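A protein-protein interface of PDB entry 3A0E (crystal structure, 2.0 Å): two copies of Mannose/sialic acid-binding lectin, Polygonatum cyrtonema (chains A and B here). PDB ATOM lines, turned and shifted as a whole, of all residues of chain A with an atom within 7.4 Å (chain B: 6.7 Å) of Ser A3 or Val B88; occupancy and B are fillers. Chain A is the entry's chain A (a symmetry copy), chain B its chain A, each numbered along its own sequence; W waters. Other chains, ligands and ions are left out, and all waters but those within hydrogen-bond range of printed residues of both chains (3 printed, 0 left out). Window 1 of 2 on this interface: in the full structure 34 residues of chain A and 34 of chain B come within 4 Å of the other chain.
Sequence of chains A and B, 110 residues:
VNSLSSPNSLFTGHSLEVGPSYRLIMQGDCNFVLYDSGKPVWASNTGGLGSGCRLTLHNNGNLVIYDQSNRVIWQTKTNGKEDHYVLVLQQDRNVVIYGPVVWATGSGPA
Water W1 bridges the side-chain amide nitrogen (NE2) of Gln B91 (2.6 Å) and the backbone carbonyl oxygen (O) of Ser A3 (2.7 Å).
Water W3 lies within hydrogen-bond range of OG of Ser A5, OG of Ser A3 and OE1 of Gln B91.
Water W2 bridges the backbone NH of Ser A5 and the side-chain amide nitrogen of Gln B91.
The side-chain amide oxygen (OD1) of Asn A2 sits close to the side-chain amide oxygen (OD1) of Asn B2 (2.6 Å).
ND2 of Asn B2 sits at hydrogen-bond distance from OG of Ser A3, 2.8 Å away.
OG of Ser B3 sits at hydrogen-bond distance from ND2 of Asn A2.
The side-chain hydroxyl of Ser A5 lies within hydrogen-bond range of the side-chain amide oxygen of Gln B90 (2.8 Å).
The side-chain amide oxygen (OD1) of Asn B94 is in hydrogen-bond range of the side-chain hydroxyl (OG1) of Thr A105 (3.3 Å).
The backbone NH (N) of Thr A105 is in hydrogen-bond range of the backbone carbonyl oxygen (O) of Val B95 (3.0 Å).
The backbone carbonyl oxygen of Asn B2 lies within hydrogen-bond range of the backbone NH of Leu B89, 2.9 Å away.
The backbone carbonyl oxygen of Val B86 lies within hydrogen-bond range of the backbone NH of Tyr B98 (2.8 Å).
The side-chain hydroxyl (OH) of Tyr B98 is in hydrogen-bond range of the side-chain amide oxygen (OE1) of Gln B90.
N of Glu A17 sits at hydrogen-bond distance from O of Val A1, at 2.9 Å.
The backbone NH (N) of Leu A89 lies within hydrogen-bond range of the backbone carbonyl oxygen (O) of Asn A2, 2.9 Å away.
N of Tyr A98 lies within hydrogen-bond range of O of Val A86 (2.8 Å).
Asn B2 touches its own counterpart, Asn A2.
Ser A3 touches Val B88, and with the chains exchanged Val A88 touches Ser B3.
Val B86 touches its own counterpart, Val A86.
Tyr A98 touches its own counterpart, Tyr B98.
10 positions are printed for both chains.
Of the 15 pairs that touch across the chains among the printed residues, 9 have their exchanged pair printed and touching as well.
Leu A10 touches none of the printed residues of chain B.
Of the printed residues of chain B, Val A86 touches Val B86 (3.7 Å) and Tyr B98 (3.5 Å).
Of the printed residues of chain A, Asn B2 touches Val A1, Asn A2 and Ser A3.
Of chain A, only Ser A3 (3.5 Å) comes within 4 Å of Val B88.
The nearest residue of chain A that does not touch Val B88 is Val A86 (4.3 Å).
The nearest printed residue of chain A that does not touch Tyr B98 is Ser A5 (4.1 Å).
Val A1 touches Asn B2.
Val A1 touches Gln B91.
OG of Ser A3 touches CG1 of Val B88 (3.5 Å).
Ser A3 touches Gln B91.
CG1 of Val B86 touches CG1 of Val A86, 3.7 Å away.
Val A86 touches Tyr B98 (CG1 to CD1, 3.5 Å).
Val A88 touches Ser B3.
Val B86 touches Tyr A98 (CG1 to CD1, 3.5 Å).
Tyr A98 touches Tyr B98.
Printed residues of chain B that touch a printed residue of chain A: Asn B2, Ser B3, Val B86, Val B88, Gln B90, Gln B91, Asn B94, Val B95 and Tyr B98.
Of the 16 printed residues of chain A, 8 touch a printed residue of chain B.
Printed residues of chain A that touch a printed residue of chain B: Val A1, Asn A2, Ser A3, Ser A5, Val A86, Val A88, Tyr A98 and Thr A105.
Among the printed residues, no Asp or Glu carboxylate lies within 4 Å of a Lys or Arg side-chain nitrogen of the other chain.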
ATOM      1  N   VAL A   1      -2.323 -12.474  24.737  1.00  0.00           N
ATOM      2  CA  VAL A   1      -1.419 -11.405  24.223  1.00  0.00           C
ATOM      3  C   VAL A   1      -1.635 -10.146  25.046  1.00  0.00           C
ATOM      4  O   VAL A   1      -2.766  -9.838  25.425  1.00  0.00           O
ATOM      5  CB  VAL A   1      -1.719 -11.094  22.734  1.00  0.00           C
ATOM      6  CG1 VAL A   1      -3.143 -10.568  22.582  1.00  0.00           C
ATOM      7  CG2 VAL A   1      -0.728 -10.080  22.203  1.00  0.00           C
ATOM      8  N   ASN A   2      -0.560  -9.419  25.339  1.00  0.00           N
ATOM      9  CA  ASN A   2      -0.702  -8.192  26.119  1.00  0.00           C
ATOM     10  C   ASN A   2      -0.177  -6.963  25.383  1.00  0.00           C
ATOM     11  O   ASN A   2       0.179  -5.968  26.008  1.00  0.00           O
ATOM     12  CB  ASN A   2       0.003  -8.321  27.471  1.00  0.00           C
ATOM     13  CG  ASN A   2       1.486  -8.604  27.335  1.00  0.00           C
ATOM     14  OD1 ASN A   2       1.884  -9.674  26.878  1.00  0.00           O
ATOM     15  ND2 ASN A   2       2.310  -7.642  27.728  1.00  0.00           N
ATOM     16  N   SER A   3      -0.145  -7.032  24.055  1.00  0.00           N
ATOM     17  CA  SER A   3       0.336  -5.915  23.251  1.00  0.00           C
ATOM     18  C   SER A   3      -0.459  -5.748  21.963  1.00  0.00           C
ATOM     19  O   SER A   3      -1.063  -6.698  21.460  1.00  0.00           O
ATOM     20  CB  SER A   3       1.814  -6.118  22.891  1.00  0.00           C
ATOM     21  OG  SER A   3       1.974  -7.211  21.995  1.00  0.00           O
ATOM     22  N   LEU A   4      -0.452  -4.525  21.439  1.00  0.00           N
ATOM     23  CA  LEU A   4      -1.125  -4.196  20.190  1.00  0.00           C
ATOM     24  C   LEU A   4      -0.134  -3.344  19.407  1.00  0.00           C
ATOM     25  O   LEU A   4       0.234  -2.258  19.846  1.00  0.00           O
ATOM     26  CB  LEU A   4      -2.404  -3.389  20.440  1.00  0.00           C
ATOM     27  CG  LEU A   4      -3.124  -2.887  19.175  1.00  0.00           C
ATOM     28  CD1 LEU A   4      -3.740  -4.068  18.415  1.00  0.00           C
ATOM     29  CD2 LEU A   4      -4.212  -1.895  19.569  1.00  0.00           C
ATOM     30  N   SER A   5       0.305  -3.841  18.256  1.00  0.00           N
ATOM     31  CA  SER A   5       1.264  -3.109  17.440  1.00  0.00           C
ATOM     32  C   SER A   5       0.584  -2.336  16.316  1.00  0.00           C
ATOM     33  O   SER A   5      -0.334  -2.843  15.668  1.00  0.00           O
ATOM     34  CB  SER A   5       2.293  -4.079  16.851  1.00  0.00           C
ATOM     35  OG  SER A   5       3.011  -4.738  17.881  1.00  0.00           O
ATOM     36  N   LEU A  10      -7.760  -3.340  18.166  1.00  0.00           N
ATOM     37  CA  LEU A  10      -8.284  -4.272  19.150  1.00  0.00           C
ATOM     38  C   LEU A  10      -9.775  -4.095  18.888  1.00  0.00           C
ATOM     39  O   LEU A  10     -10.319  -3.015  19.115  1.00  0.00           O
ATOM     40  CB  LEU A  10      -7.932  -3.815  20.571  1.00  0.00           C
ATOM     41  CG  LEU A  10      -8.358  -4.733  21.722  1.00  0.00           C
ATOM     42  CD1 LEU A  10      -7.715  -6.107  21.561  1.00  0.00           C
ATOM     43  CD2 LEU A  10      -7.939  -4.102  23.043  1.00  0.00           C
ATOM     44  N   SER A  15      -9.537  -8.214  24.222  1.00  0.00           N
ATOM     45  CA  SER A  15      -8.707  -7.647  25.277  1.00  0.00           C
ATOM     46  C   SER A  15      -7.223  -7.986  25.195  1.00  0.00           C
ATOM     47  O   SER A  15      -6.802  -8.880  24.461  1.00  0.00           O
ATOM     48  CB  SER A  15      -9.195  -8.152  26.642  1.00  0.00           C
ATOM     49  OG  SER A  15     -10.608  -8.219  26.723  1.00  0.00           O
ATOM     50  N   LEU A  16      -6.442  -7.243  25.968  1.00  0.00           N
ATOM     51  CA  LEU A  16      -5.018  -7.500  26.114  1.00  0.00           C
ATOM     52  C   LEU A  16      -5.042  -8.024  27.538  1.00  0.00           C
ATOM     53  O   LEU A  16      -5.788  -7.502  28.376  1.00  0.00           O
ATOM     54  CB  LEU A  16      -4.191  -6.216  26.041  1.00  0.00           C
ATOM     55  CG  LEU A  16      -4.172  -5.525  24.678  1.00  0.00           C
ATOM     56  CD1 LEU A  16      -3.102  -4.438  24.680  1.00  0.00           C
ATOM     57  CD2 LEU A  16      -3.889  -6.550  23.584  1.00  0.00           C
ATOM     58  N   GLU A  17      -4.261  -9.056  27.826  1.00  0.00           N
ATOM     59  CA  GLU A  17      -4.274  -9.615  29.166  1.00  0.00           C
ATOM     60  C   GLU A  17      -2.911 -10.040  29.670  1.00  0.00           C
ATOM     61  O   GLU A  17      -2.059 -10.507  28.911  1.00  0.00           O
ATOM     62  CB  GLU A  17      -5.230 -10.815  29.218  1.00  0.00           C
ATOM     63  CG  GLU A  17      -6.688 -10.458  28.943  1.00  0.00           C
ATOM     64  CD  GLU A  17      -7.586 -11.675  28.783  1.00  0.00           C
ATOM     65  OE1 GLU A  17      -8.806 -11.489  28.581  1.00  0.00           O
ATOM     66  OE2 GLU A  17      -7.075 -12.815  28.856  1.00  0.00           O
ATOM     67  N   VAL A  18      -2.721  -9.848  30.970  1.00  0.00           N
ATOM     68  CA  VAL A  18      -1.506 -10.221  31.672  1.00  0.00           C
ATOM     69  C   VAL A  18      -2.046 -10.945  32.890  1.00  0.00           C
ATOM     70  O   VAL A  18      -2.461 -10.318  33.864  1.00  0.00           O
ATOM     71  CB  VAL A  18      -0.694  -8.990  32.125  1.00  0.00           C
ATOM     72  CG1 VAL A  18       0.418  -9.418  33.077  1.00  0.00           C
ATOM     73  CG2 VAL A  18      -0.098  -8.298  30.921  1.00  0.00           C
ATOM     74  N   VAL A  86       3.890   0.509  19.605  1.00  0.00           N
ATOM     75  CA  VAL A  86       3.211  -0.589  20.270  1.00  0.00           C
ATOM     76  C   VAL A  86       2.549  -0.106  21.555  1.00  0.00           C
ATOM     77  O   VAL A  86       3.050   0.802  22.223  1.00  0.00           O
ATOM     78  CB  VAL A  86       4.190  -1.744  20.613  1.00  0.00           C
ATOM     79  CG1 VAL A  86       5.177  -1.303  21.693  1.00  0.00           C
ATOM     80  CG2 VAL A  86       3.402  -2.973  21.075  1.00  0.00           C
ATOM     81  N   LEU A  87       1.405  -0.706  21.868  1.00  0.00           N
ATOM     82  CA  LEU A  87       0.649  -0.409  23.082  1.00  0.00           C
ATOM     83  C   LEU A  87       0.810  -1.658  23.933  1.00  0.00           C
ATOM     84  O   LEU A  87       0.540  -2.761  23.461  1.00  0.00           O
ATOM     85  CB  LEU A  87      -0.833  -0.212  22.765  1.00  0.00           C
ATOM     86  CG  LEU A  87      -1.721  -0.071  24.006  1.00  0.00           C
ATOM     87  CD1 LEU A  87      -1.376   1.231  24.726  1.00  0.00           C
ATOM     88  CD2 LEU A  87      -3.190  -0.084  23.602  1.00  0.00           C
ATOM     89  N   VAL A  88       1.221  -1.494  25.185  1.00  0.00           N
ATOM     90  CA  VAL A  88       1.445  -2.648  26.040  1.00  0.00           C
ATOM     91  C   VAL A  88       0.834  -2.596  27.435  1.00  0.00           C
ATOM     92  O   VAL A  88       0.981  -1.607  28.160  1.00  0.00           O
ATOM     93  CB  VAL A  88       2.964  -2.897  26.216  1.00  0.00           C
ATOM     94  CG1 VAL A  88       3.203  -4.128  27.072  1.00  0.00           C
ATOM     95  CG2 VAL A  88       3.633  -3.045  24.854  1.00  0.00           C
ATOM     96  N   LEU A  89       0.131  -3.664  27.796  1.00  0.00           N
ATOM     97  CA  LEU A  89      -0.428  -3.794  29.138  1.00  0.00           C
ATOM     98  C   LEU A  89       0.703  -4.530  29.856  1.00  0.00           C
ATOM     99  O   LEU A  89       0.963  -5.702  29.580  1.00  0.00           O
ATOM    100  CB  LEU A  89      -1.694  -4.655  29.131  1.00  0.00           C
ATOM    101  CG  LEU A  89      -2.111  -5.185  30.508  1.00  0.00           C
ATOM    102  CD1 LEU A  89      -2.282  -4.022  31.486  1.00  0.00           C
ATOM    103  CD2 LEU A  89      -3.400  -5.990  30.373  1.00  0.00           C
ATOM    104  N   TYR A  98       4.827   2.716  23.300  1.00  0.00           N
ATOM    105  CA  TYR A  98       6.265   2.869  23.056  1.00  0.00           C
ATOM    106  C   TYR A  98       6.548   2.980  21.566  1.00  0.00           C
ATOM    107  O   TYR A  98       5.870   2.357  20.748  1.00  0.00           O
ATOM    108  CB  TYR A  98       7.061   1.664  23.561  1.00  0.00           C
ATOM    109  CG  TYR A  98       7.089   1.468  25.053  1.00  0.00           C
ATOM    110  CD1 TYR A  98       6.136   0.671  25.688  1.00  0.00           C
ATOM    111  CD2 TYR A  98       8.114   2.018  25.824  1.00  0.00           C
ATOM    112  CE1 TYR A  98       6.212   0.416  27.056  1.00  0.00           C
ATOM    113  CE2 TYR A  98       8.196   1.773  27.194  1.00  0.00           C
ATOM    114  CZ  TYR A  98       7.244   0.969  27.800  1.00  0.00           C
ATOM    115  OH  TYR A  98       7.337   0.702  29.145  1.00  0.00           O
ATOM    116  N   THR A 105      14.299  -8.073  14.841  1.00  0.00           N
ATOM    117  CA  THR A 105      14.945  -9.285  14.348  1.00  0.00           C
ATOM    118  C   THR A 105      14.653  -9.488  12.871  1.00  0.00           C
ATOM    119  O   THR A 105      15.473 -10.040  12.138  1.00  0.00           O
ATOM    120  CB  THR A 105      14.431 -10.528  15.074  1.00  0.00           C
ATOM    121  OG1 THR A 105      13.009 -10.606  14.910  1.00  0.00           O
ATOM    122  CG2 THR A 105      14.783 -10.478  16.555  1.00  0.00           C
ATOM    123  N   ASN B   2       3.930 -11.590  26.225  1.00  0.00           N
ATOM    124  CA  ASN B   2       4.772 -11.533  25.033  1.00  0.00           C
ATOM    125  C   ASN B   2       5.614 -10.263  24.967  1.00  0.00           C
ATOM    126  O   ASN B   2       6.030  -9.847  23.889  1.00  0.00           O
ATOM    127  CB  ASN B   2       3.929 -11.658  23.762  1.00  0.00           C
ATOM    128  CG  ASN B   2       2.893 -10.560  23.637  1.00  0.00           C
ATOM    129  OD1 ASN B   2       1.943 -10.496  24.417  1.00  0.00           O
ATOM    130  ND2 ASN B   2       3.071  -9.687  22.655  1.00  0.00           N
ATOM    131  N   SER B   3       5.875  -9.659  26.124  1.00  0.00           N
ATOM    132  CA  SER B   3       6.671  -8.439  26.177  1.00  0.00           C
ATOM    133  C   SER B   3       7.580  -8.399  27.399  1.00  0.00           C
ATOM    134  O   SER B   3       7.311  -9.044  28.414  1.00  0.00           O
ATOM    135  CB  SER B   3       5.756  -7.209  26.207  1.00  0.00           C
ATOM    136  OG  SER B   3       5.036  -7.140  27.432  1.00  0.00           O
ATOM    137  N   LEU B   4       8.661  -7.632  27.284  1.00  0.00           N
ATOM    138  CA  LEU B   4       9.617  -7.445  28.368  1.00  0.00           C
ATOM    139  C   LEU B   4       9.908  -5.950  28.397  1.00  0.00           C
ATOM    140  O   LEU B   4      10.435  -5.400  27.433  1.00  0.00           O
ATOM    141  CB  LEU B   4      10.917  -8.213  28.105  1.00  0.00           C
ATOM    142  CG  LEU B   4      12.038  -7.981  29.135  1.00  0.00           C
ATOM    143  CD1 LEU B   4      11.661  -8.617  30.478  1.00  0.00           C
ATOM    144  CD2 LEU B   4      13.337  -8.587  28.617  1.00  0.00           C
ATOM    145  N   LEU B  16       8.843 -15.537  26.164  1.00  0.00           N
ATOM    146  CA  LEU B  16       7.789 -14.603  25.801  1.00  0.00           C
ATOM    147  C   LEU B  16       7.038 -15.497  24.832  1.00  0.00           C
ATOM    148  O   LEU B  16       7.662 -16.240  24.065  1.00  0.00           O
ATOM    149  CB  LEU B  16       8.334 -13.376  25.069  1.00  0.00           C
ATOM    150  CG  LEU B  16       9.204 -12.443  25.910  1.00  0.00           C
ATOM    151  CD1 LEU B  16       9.438 -11.145  25.143  1.00  0.00           C
ATOM    152  CD2 LEU B  16       8.515 -12.159  27.242  1.00  0.00           C
ATOM    153  N   VAL B  18       3.426 -16.036  22.159  1.00  0.00           N
ATOM    154  CA  VAL B  18       2.261 -15.569  21.426  1.00  0.00           C
ATOM    155  C   VAL B  18       1.701 -16.857  20.854  1.00  0.00           C
ATOM    156  O   VAL B  18       2.185 -17.359  19.841  1.00  0.00           O
ATOM    157  CB  VAL B  18       2.642 -14.617  20.273  1.00  0.00           C
ATOM    158  CG1 VAL B  18       1.432 -14.369  19.379  1.00  0.00           C
ATOM    159  CG2 VAL B  18       3.141 -13.307  20.835  1.00  0.00           C
ATOM    160  N   LEU B  24       9.684 -17.285  22.337  1.00  0.00           N
ATOM    161  CA  LEU B  24      10.997 -16.639  22.368  1.00  0.00           C
ATOM    162  C   LEU B  24      11.563 -16.948  23.751  1.00  0.00           C
ATOM    163  O   LEU B  24      11.125 -16.382  24.750  1.00  0.00           O
ATOM    164  CB  LEU B  24      10.846 -15.129  22.172  1.00  0.00           C
ATOM    165  CG  LEU B  24      12.126 -14.295  22.137  1.00  0.00           C
ATOM    166  CD1 LEU B  24      13.034 -14.770  20.999  1.00  0.00           C
ATOM    167  CD2 LEU B  24      11.758 -12.831  21.954  1.00  0.00           C
ATOM    168  N   LEU B  57      16.693  -5.865  28.942  1.00  0.00           N
ATOM    169  CA  LEU B  57      16.433  -4.702  28.103  1.00  0.00           C
ATOM    170  C   LEU B  57      16.679  -3.513  29.026  1.00  0.00           C
ATOM    171  O   LEU B  57      16.039  -3.393  30.076  1.00  0.00           O
ATOM    172  CB  LEU B  57      14.982  -4.677  27.611  1.00  0.00           C
ATOM    173  CG  LEU B  57      14.634  -3.438  26.776  1.00  0.00           C
ATOM    174  CD1 LEU B  57      15.556  -3.373  25.555  1.00  0.00           C
ATOM    175  CD2 LEU B  57      13.169  -3.483  26.348  1.00  0.00           C
ATOM    176  N   VAL B  86      10.557  -1.258  25.457  1.00  0.00           N
ATOM    177  CA  VAL B  86       9.923  -2.561  25.562  1.00  0.00           C
ATOM    178  C   VAL B  86      10.357  -3.459  24.410  1.00  0.00           C
ATOM    179  O   VAL B  86      10.611  -2.987  23.300  1.00  0.00           O
ATOM    180  CB  VAL B  86       8.375  -2.446  25.553  1.00  0.00           C
ATOM    181  CG1 VAL B  86       7.883  -1.983  24.183  1.00  0.00           C
ATOM    182  CG2 VAL B  86       7.753  -3.796  25.919  1.00  0.00           C
ATOM    183  N   LEU B  87      10.468  -4.750  24.705  1.00  0.00           N
ATOM    184  CA  LEU B  87      10.828  -5.769  23.722  1.00  0.00           C
ATOM    185  C   LEU B  87       9.549  -6.566  23.528  1.00  0.00           C
ATOM    186  O   LEU B  87       8.962  -7.031  24.503  1.00  0.00           O
ATOM    187  CB  LEU B  87      11.912  -6.697  24.274  1.00  0.00           C
ATOM    188  CG  LEU B  87      12.221  -7.897  23.372  1.00  0.00           C
ATOM    189  CD1 LEU B  87      12.858  -7.403  22.076  1.00  0.00           C
ATOM    190  CD2 LEU B  87      13.154  -8.863  24.091  1.00  0.00           C
ATOM    191  N   VAL B  88       9.128  -6.749  22.282  1.00  0.00           N
ATOM    192  CA  VAL B  88       7.885  -7.458  22.025  1.00  0.00           C
ATOM    193  C   VAL B  88       7.927  -8.551  20.964  1.00  0.00           C
ATOM    194  O   VAL B  88       8.433  -8.347  19.856  1.00  0.00           O
ATOM    195  CB  VAL B  88       6.776  -6.460  21.608  1.00  0.00           C
ATOM    196  CG1 VAL B  88       5.464  -7.191  21.382  1.00  0.00           C
ATOM    197  CG2 VAL B  88       6.618  -5.377  22.671  1.00  0.00           C
ATOM    198  N   LEU B  89       7.407  -9.720  21.321  1.00  0.00           N
ATOM    199  CA  LEU B  89       7.290 -10.827  20.376  1.00  0.00           C
ATOM    200  C   LEU B  89       5.888 -10.586  19.817  1.00  0.00           C
ATOM    201  O   LEU B  89       4.894 -10.757  20.524  1.00  0.00           O
ATOM    202  CB  LEU B  89       7.345 -12.177  21.093  1.00  0.00           C
ATOM    203  CG  LEU B  89       6.828 -13.360  20.265  1.00  0.00           C
ATOM    204  CD1 LEU B  89       7.588 -13.445  18.942  1.00  0.00           C
ATOM    205  CD2 LEU B  89       6.973 -14.647  21.072  1.00  0.00           C
ATOM    206  N   GLN B  90       5.810 -10.179  18.556  1.00  0.00           N
ATOM    207  CA  GLN B  90       4.526  -9.863  17.940  1.00  0.00           C
ATOM    208  C   GLN B  90       3.782 -11.019  17.289  1.00  0.00           C
ATOM    209  O   GLN B  90       4.364 -12.057  16.967  1.00  0.00           O
ATOM    210  CB  GLN B  90       4.726  -8.743  16.917  1.00  0.00           C
ATOM    211  CG  GLN B  90       5.267  -7.465  17.536  1.00  0.00           C
ATOM    212  CD  GLN B  90       5.460  -6.350  16.531  1.00  0.00           C
ATOM    213  OE1 GLN B  90       5.560  -5.185  16.903  1.00  0.00           O
ATOM    214  NE2 GLN B  90       5.527  -6.703  15.251  1.00  0.00           N
ATOM    215  N   GLN B  91       2.481 -10.832  17.098  1.00  0.00           N
ATOM    216  CA  GLN B  91       1.672 -11.864  16.469  1.00  0.00           C
ATOM    217  C   GLN B  91       2.095 -12.090  15.023  1.00  0.00           C
ATOM    218  O   GLN B  91       1.806 -13.140  14.465  1.00  0.00           O
ATOM    219  CB  GLN B  91       0.181 -11.521  16.538  1.00  0.00           C
ATOM    220  CG  GLN B  91      -0.152 -10.050  16.436  1.00  0.00           C
ATOM    221  CD  GLN B  91       0.117  -9.306  17.729  1.00  0.00           C
ATOM    222  OE1 GLN B  91       1.268  -9.048  18.086  1.00  0.00           O
ATOM    223  NE2 GLN B  91      -0.948  -8.968  18.448  1.00  0.00           N
ATOM    224  N   ASN B  94       7.434 -11.000  14.319  1.00  0.00           N
ATOM    225  CA  ASN B  94       8.615 -10.146  14.390  1.00  0.00           C
ATOM    226  C   ASN B  94       8.898  -9.891  15.877  1.00  0.00           C
ATOM    227  O   ASN B  94       7.980  -9.917  16.697  1.00  0.00           O
ATOM    228  CB  ASN B  94       8.360  -8.816  13.666  1.00  0.00           C
ATOM    229  CG  ASN B  94       9.643  -8.149  13.190  1.00  0.00           C
ATOM    230  OD1 ASN B  94      10.740  -8.678  13.378  1.00  0.00           O
ATOM    231  ND2 ASN B  94       9.509  -6.985  12.560  1.00  0.00           N
ATOM    232  N   VAL B  95      10.167  -9.685  16.221  1.00  0.00           N
ATOM    233  CA  VAL B  95      10.572  -9.401  17.601  1.00  0.00           C
ATOM    234  C   VAL B  95      11.135  -7.988  17.527  1.00  0.00           C
ATOM    235  O   VAL B  95      12.115  -7.736  16.829  1.00  0.00           O
ATOM    236  CB  VAL B  95      11.646 -10.398  18.088  1.00  0.00           C
ATOM    237  CG1 VAL B  95      12.195  -9.971  19.444  1.00  0.00           C
ATOM    238  CG2 VAL B  95      11.026 -11.793  18.191  1.00  0.00           C
ATOM    239  N   VAL B  96      10.525  -7.066  18.262  1.00  0.00           N
ATOM    240  CA  VAL B  96      10.916  -5.668  18.160  1.00  0.00           C
ATOM    241  C   VAL B  96      11.114  -4.906  19.459  1.00  0.00           C
ATOM    242  O   VAL B  96      10.412  -5.133  20.438  1.00  0.00           O
ATOM    243  CB  VAL B  96       9.839  -4.914  17.338  1.00  0.00           C
ATOM    244  CG1 VAL B  96      10.306  -3.507  17.002  1.00  0.00           C
ATOM    245  CG2 VAL B  96       9.496  -5.708  16.083  1.00  0.00           C
ATOM    246  N   ILE B  97      12.077  -3.990  19.447  1.00  0.00           N
ATOM    247  CA  ILE B  97      12.334  -3.127  20.591  1.00  0.00           C
ATOM    248  C   ILE B  97      11.733  -1.768  20.227  1.00  0.00           C
ATOM    249  O   ILE B  97      12.089  -1.190  19.196  1.00  0.00           O
ATOM    250  CB  ILE B  97      13.843  -2.921  20.845  1.00  0.00           C
ATOM    251  CG1 ILE B  97      14.495  -4.241  21.267  1.00  0.00           C
ATOM    252  CG2 ILE B  97      14.039  -1.859  21.925  1.00  0.00           C
ATOM    253  CD1 ILE B  97      15.993  -4.134  21.487  1.00  0.00           C
ATOM    254  N   TYR B  98      10.815  -1.278  21.059  1.00  0.00           N
ATOM    255  CA  TYR B  98      10.171   0.021  20.838  1.00  0.00           C
ATOM    256  C   TYR B  98      10.468   0.971  21.987  1.00  0.00           C
ATOM    257  O   TYR B  98      10.576   0.552  23.140  1.00  0.00           O
ATOM    258  CB  TYR B  98       8.648  -0.103  20.759  1.00  0.00           C
ATOM    259  CG  TYR B  98       8.106  -0.849  19.570  1.00  0.00           C
ATOM    260  CD1 TYR B  98       7.872  -2.221  19.631  1.00  0.00           C
ATOM    261  CD2 TYR B  98       7.754  -0.167  18.403  1.00  0.00           C
ATOM    262  CE1 TYR B  98       7.287  -2.898  18.561  1.00  0.00           C
ATOM    263  CE2 TYR B  98       7.173  -0.835  17.326  1.00  0.00           C
ATOM    264  CZ  TYR B  98       6.940  -2.197  17.416  1.00  0.00           C
ATOM    265  OH  TYR B  98       6.341  -2.855  16.367  1.00  0.00           O
HETATM  266  O   HOH W   1      -2.829  -7.590  19.565  1.00  0.00           O
HETATM  267  O   HOH W   2      -0.632  -6.323  17.303  1.00  0.00           O
HETATM  268  O   HOH W   3       1.968  -6.599  19.365  1.00  0.00           O
